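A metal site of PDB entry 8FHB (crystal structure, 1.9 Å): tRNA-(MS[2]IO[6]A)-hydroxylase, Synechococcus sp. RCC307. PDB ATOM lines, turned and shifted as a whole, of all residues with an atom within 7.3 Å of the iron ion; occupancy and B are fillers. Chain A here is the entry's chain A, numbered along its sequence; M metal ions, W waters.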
ATOM      1  N   HIS A  44       7.744 -10.395 -36.669  1.00  0.00           N
ATOM      2  CA  HIS A  44       8.505  -9.984 -35.519  1.00  0.00           C
ATOM      3  C   HIS A  44       7.679  -9.151 -34.552  1.00  0.00           C
ATOM      4  O   HIS A  44       7.714  -9.346 -33.318  1.00  0.00           O
ATOM      5  CB  HIS A  44       9.832  -9.304 -35.942  1.00  0.00           C
ATOM      6  CG  HIS A  44      10.661  -8.962 -34.766  1.00  0.00           C
ATOM      7  ND1 HIS A  44      11.420  -7.821 -34.723  1.00  0.00           N
ATOM      8  CD2 HIS A  44      10.886  -9.577 -33.606  1.00  0.00           C
ATOM      9  CE1 HIS A  44      11.947  -7.700 -33.515  1.00  0.00           C
ATOM     10  NE2 HIS A  44      11.621  -8.727 -32.826  1.00  0.00           N
ATOM     11  N   CYS A  47       5.482 -11.386 -32.787  1.00  0.00           N
ATOM     12  CA  CYS A  47       6.247 -12.207 -31.845  1.00  0.00           C
ATOM     13  C   CYS A  47       6.518 -11.437 -30.559  1.00  0.00           C
ATOM     14  O   CYS A  47       6.441 -12.036 -29.494  1.00  0.00           O
ATOM     15  CB  CYS A  47       7.566 -12.696 -32.427  1.00  0.00           C
ATOM     16  SG  CYS A  47       7.363 -13.949 -33.703  1.00  0.00           S
ATOM     17  N   GLU A  48       6.952 -10.155 -30.647  1.00  0.00           N
ATOM     18  CA  GLU A  48       7.181  -9.378 -29.434  1.00  0.00           C
ATOM     19  C   GLU A  48       5.964  -9.379 -28.525  1.00  0.00           C
ATOM     20  O   GLU A  48       6.069  -9.428 -27.264  1.00  0.00           O
ATOM     21  CB  GLU A  48       7.594  -7.928 -29.734  1.00  0.00           C
ATOM     22  CG  GLU A  48       8.916  -7.844 -30.483  1.00  0.00           C
ATOM     23  CD  GLU A  48      10.175  -8.155 -29.672  1.00  0.00           C
ATOM     24  OE1 GLU A  48      10.029  -8.422 -28.470  1.00  0.00           O
ATOM     25  OE2 GLU A  48      11.326  -8.012 -30.175  1.00  0.00           O
ATOM     26  N   ARG A  49       4.843  -9.103 -29.159  1.00  0.00           N
ATOM     27  CA  ARG A  49       3.570  -9.003 -28.440  1.00  0.00           C
ATOM     28  C   ARG A  49       3.180 -10.361 -27.826  1.00  0.00           C
ATOM     29  O   ARG A  49       2.800 -10.408 -26.652  1.00  0.00           O
ATOM     30  CB  ARG A  49       2.488  -8.520 -29.405  1.00  0.00           C
ATOM     31  CG  ARG A  49       1.296  -7.926 -28.680  1.00  0.00           C
ATOM     32  CD  ARG A  49       0.468  -7.025 -29.586  1.00  0.00           C
ATOM     33  NE  ARG A  49       0.175  -7.593 -30.920  1.00  0.00           N
ATOM     34  CZ  ARG A  49      -0.690  -7.088 -31.801  1.00  0.00           C
ATOM     35  NH1 ARG A  49      -1.349  -5.947 -31.567  1.00  0.00           N
ATOM     36  NH2 ARG A  49      -0.851  -7.739 -32.938  1.00  0.00           N
ATOM     37  N   ALA A  51       5.335 -12.650 -26.959  1.00  0.00           N
ATOM     38  CA  ALA A  51       6.315 -12.820 -25.887  1.00  0.00           C
ATOM     39  C   ALA A  51       5.842 -12.111 -24.586  1.00  0.00           C
ATOM     40  O   ALA A  51       5.942 -12.651 -23.467  1.00  0.00           O
ATOM     41  CB  ALA A  51       7.725 -12.424 -26.350  1.00  0.00           C
ATOM     42  N   LEU A  75       9.587  -7.880 -17.786  1.00  0.00           N
ATOM     43  CA  LEU A  75       9.811  -8.463 -19.097  1.00  0.00           C
ATOM     44  C   LEU A  75       8.640  -8.168 -20.052  1.00  0.00           C
ATOM     45  O   LEU A  75       8.870  -7.833 -21.212  1.00  0.00           O
ATOM     46  CB  LEU A  75       9.995  -9.962 -18.991  1.00  0.00           C
ATOM     47  CG  LEU A  75      10.186 -10.706 -20.319  1.00  0.00           C
ATOM     48  CD1 LEU A  75      11.366 -10.176 -21.055  1.00  0.00           C
ATOM     49  CD2 LEU A  75      10.316 -12.170 -20.042  1.00  0.00           C
ATOM     50  N   GLU A  78       8.884  -4.682 -21.260  1.00  0.00           N
ATOM     51  CA  GLU A  78       9.934  -4.505 -22.241  1.00  0.00           C
ATOM     52  C   GLU A  78       9.559  -5.097 -23.584  1.00  0.00           C
ATOM     53  O   GLU A  78       9.843  -4.524 -24.671  1.00  0.00           O
ATOM     54  CB  GLU A  78      11.238  -5.044 -21.612  1.00  0.00           C
ATOM     55  CG  GLU A  78      12.326  -4.927 -22.625  1.00  0.00           C
ATOM     56  CD  GLU A  78      13.705  -5.431 -22.235  1.00  0.00           C
ATOM     57  OE1 GLU A  78      13.935  -6.679 -22.244  1.00  0.00           O
ATOM     58  OE2 GLU A  78      14.527  -4.580 -21.969  1.00  0.00           O
ATOM     59  N   GLU A  79       8.853  -6.251 -23.562  1.00  0.00           N
ATOM     60  CA  GLU A  79       8.448  -6.836 -24.820  1.00  0.00           C
ATOM     61  C   GLU A  79       7.447  -5.914 -25.542  1.00  0.00           C
ATOM     62  O   GLU A  79       7.420  -5.890 -26.773  1.00  0.00           O
ATOM     63  CB  GLU A  79       7.949  -8.277 -24.561  1.00  0.00           C
ATOM     64  CG  GLU A  79       9.068  -9.224 -24.130  1.00  0.00           C
ATOM     65  CD  GLU A  79      10.158  -9.357 -25.171  1.00  0.00           C
ATOM     66  OE1 GLU A  79      10.247 -10.472 -25.760  1.00  0.00           O
ATOM     67  OE2 GLU A  79      11.023  -8.403 -25.317  1.00  0.00           O
ATOM     68  N   LEU A  80       6.547  -5.263 -24.808  1.00  0.00           N
ATOM     69  CA  LEU A  80       5.633  -4.298 -25.427  1.00  0.00           C
ATOM     70  C   LEU A  80       6.376  -3.050 -25.923  1.00  0.00           C
ATOM     71  O   LEU A  80       6.057  -2.499 -26.961  1.00  0.00           O
ATOM     72  CB  LEU A  80       4.560  -3.999 -24.393  1.00  0.00           C
ATOM     73  CG  LEU A  80       3.575  -5.166 -24.182  1.00  0.00           C
ATOM     74  CD1 LEU A  80       2.704  -4.922 -22.985  1.00  0.00           C
ATOM     75  CD2 LEU A  80       2.739  -5.454 -25.422  1.00  0.00           C
ATOM     76  N   GLU A  81       7.377  -2.582 -25.189  1.00  0.00           N
ATOM     77  CA  GLU A  81       8.182  -1.485 -25.741  1.00  0.00           C
ATOM     78  C   GLU A  81       8.853  -1.935 -27.058  1.00  0.00           C
ATOM     79  O   GLU A  81       8.853  -1.185 -28.009  1.00  0.00           O
ATOM     80  CB  GLU A  81       9.311  -1.051 -24.791  1.00  0.00           C
ATOM     81  CG  GLU A  81       8.798  -0.489 -23.488  1.00  0.00           C
ATOM     82  CD  GLU A  81       9.867  -0.321 -22.417  1.00  0.00           C
ATOM     83  OE1 GLU A  81      11.085  -0.427 -22.728  1.00  0.00           O
ATOM     84  OE2 GLU A  81       9.476  -0.284 -21.247  1.00  0.00           O
ATOM     85  N   HIS A  82       9.339  -3.184 -27.158  1.00  0.00           N
ATOM     86  CA  HIS A  82       9.893  -3.669 -28.430  1.00  0.00           C
ATOM     87  C   HIS A  82       8.843  -3.757 -29.528  1.00  0.00           C
ATOM     88  O   HIS A  82       9.068  -3.357 -30.670  1.00  0.00           O
ATOM     89  CB  HIS A  82      10.561  -5.028 -28.249  1.00  0.00           C
ATOM     90  CG  HIS A  82      11.768  -5.007 -27.370  1.00  0.00           C
ATOM     91  ND1 HIS A  82      12.433  -6.190 -27.026  1.00  0.00           N
ATOM     92  CD2 HIS A  82      12.462  -3.998 -26.806  1.00  0.00           C
ATOM     93  CE1 HIS A  82      13.467  -5.867 -26.262  1.00  0.00           C
ATOM     94  NE2 HIS A  82      13.536  -4.552 -26.192  1.00  0.00           N
ATOM     95  N   PHE A  83       7.636  -4.239 -29.160  1.00  0.00           N
ATOM     96  CA  PHE A  83       6.556  -4.254 -30.112  1.00  0.00           C
ATOM     97  C   PHE A  83       6.300  -2.828 -30.636  1.00  0.00           C
ATOM     98  O   PHE A  83       6.202  -2.591 -31.844  1.00  0.00           O
ATOM     99  CB  PHE A  83       5.270  -4.852 -29.535  1.00  0.00           C
ATOM    100  CG  PHE A  83       4.012  -4.534 -30.326  1.00  0.00           C
ATOM    101  CD1 PHE A  83       3.668  -5.279 -31.444  1.00  0.00           C
ATOM    102  CD2 PHE A  83       3.204  -3.465 -29.984  1.00  0.00           C
ATOM    103  CE1 PHE A  83       2.546  -4.979 -32.213  1.00  0.00           C
ATOM    104  CE2 PHE A  83       2.092  -3.149 -30.739  1.00  0.00           C
ATOM    105  CZ  PHE A  83       1.779  -3.890 -31.870  1.00  0.00           C
ATOM    106  N   GLU A 132      12.453 -17.509 -27.104  1.00  0.00           N
ATOM    107  CA  GLU A 132      13.264 -16.308 -26.977  1.00  0.00           C
ATOM    108  C   GLU A 132      14.724 -16.555 -27.454  1.00  0.00           C
ATOM    109  O   GLU A 132      15.298 -15.682 -28.113  1.00  0.00           O
ATOM    110  CB  GLU A 132      13.246 -15.789 -25.544  1.00  0.00           C
ATOM    111  CG  GLU A 132      13.710 -14.283 -25.451  1.00  0.00           C
ATOM    112  CD  GLU A 132      15.234 -14.197 -25.431  1.00  0.00           C
ATOM    113  OE1 GLU A 132      15.852 -13.161 -25.843  1.00  0.00           O
ATOM    114  OE2 GLU A 132      15.840 -15.227 -24.989  1.00  0.00           O
ATOM    115  N   MET A 139      17.610 -12.693 -34.691  1.00  0.00           N
ATOM    116  CA  MET A 139      17.676 -11.258 -34.643  1.00  0.00           C
ATOM    117  C   MET A 139      19.150 -10.812 -34.731  1.00  0.00           C
ATOM    118  O   MET A 139      19.443  -9.816 -35.386  1.00  0.00           O
ATOM    119  CB  MET A 139      17.012 -10.730 -33.367  1.00  0.00           C
ATOM    120  CG  MET A 139      15.487 -10.704 -33.439  1.00  0.00           C
ATOM    121  SD  MET A 139      14.878 -10.297 -31.778  1.00  0.00           S
ATOM    122  CE  MET A 139      15.322  -8.583 -31.774  1.00  0.00           C
ATOM    123  N   LEU A 158      17.357  -3.676 -30.210  1.00  0.00           N
ATOM    124  CA  LEU A 158      16.454  -4.579 -29.476  1.00  0.00           C
ATOM    125  C   LEU A 158      17.307  -5.581 -28.676  1.00  0.00           C
ATOM    126  O   LEU A 158      17.015  -5.881 -27.521  1.00  0.00           O
ATOM    127  CB  LEU A 158      15.485  -5.286 -30.428  1.00  0.00           C
ATOM    128  CG  LEU A 158      14.419  -4.421 -31.124  1.00  0.00           C
ATOM    129  CD1 LEU A 158      13.484  -5.291 -31.942  1.00  0.00           C
ATOM    130  CD2 LEU A 158      13.642  -3.589 -30.145  1.00  0.00           C
ATOM    131  N   SER A 161      19.325  -3.969 -25.305  1.00  0.00           N
ATOM    132  CA  SER A 161      18.594  -3.969 -24.042  1.00  0.00           C
ATOM    133  C   SER A 161      18.415  -5.411 -23.500  1.00  0.00           C
ATOM    134  O   SER A 161      17.302  -5.952 -23.489  1.00  0.00           O
ATOM    135  CB  SER A 161      17.273  -3.208 -24.203  1.00  0.00           C
ATOM    136  OG  SER A 161      16.517  -3.668 -25.320  1.00  0.00           O
ATOM    137  N   GLU A 162      19.558  -5.990 -23.033  1.00  0.00           N
ATOM    138  CA  GLU A 162      19.760  -7.401 -22.718  1.00  0.00           C
ATOM    139  C   GLU A 162      20.850  -7.566 -21.650  1.00  0.00           C
ATOM    140  O   GLU A 162      20.689  -7.111 -20.529  1.00  0.00           O
ATOM    141  CB  GLU A 162      20.174  -8.215 -23.961  1.00  0.00           C
ATOM    142  CG  GLU A 162      19.150  -8.272 -25.063  1.00  0.00           C
ATOM    143  CD  GLU A 162      17.987  -9.193 -24.763  1.00  0.00           C
ATOM    144  OE1 GLU A 162      18.295 -10.404 -24.599  1.00  0.00           O
ATOM    145  OE2 GLU A 162      16.804  -8.700 -24.714  1.00  0.00           O
HETATM  146 FE    FE M   1      11.677  -8.280 -27.299  1.00  0.00          FE
HETATM  147  O   HOH W   1      13.450  -9.965 -27.208  1.00  0.00           O
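The iron ion is bound by OE1 of Glu 48 (2.0 Å), OE2 of Glu 79 (2.1 Å), ND1 of His 82 (2.2 Å) and water W1 (2.4 Å).
A ring nitrogen (NE2) of His 82 sits at hydrogen-bond distance from the side-chain hydroxyl (OG) of Ser 161 (3.2 Å). The side-chain carboxylate (OE2) of Glu 48 sits at hydrogen-bond distance from a ring nitrogen (NE2) of His 44 (2.8 Å).
Three residues have an atom within 4 Å of the iron ion: Glu 48, Glu 79 and His 82.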
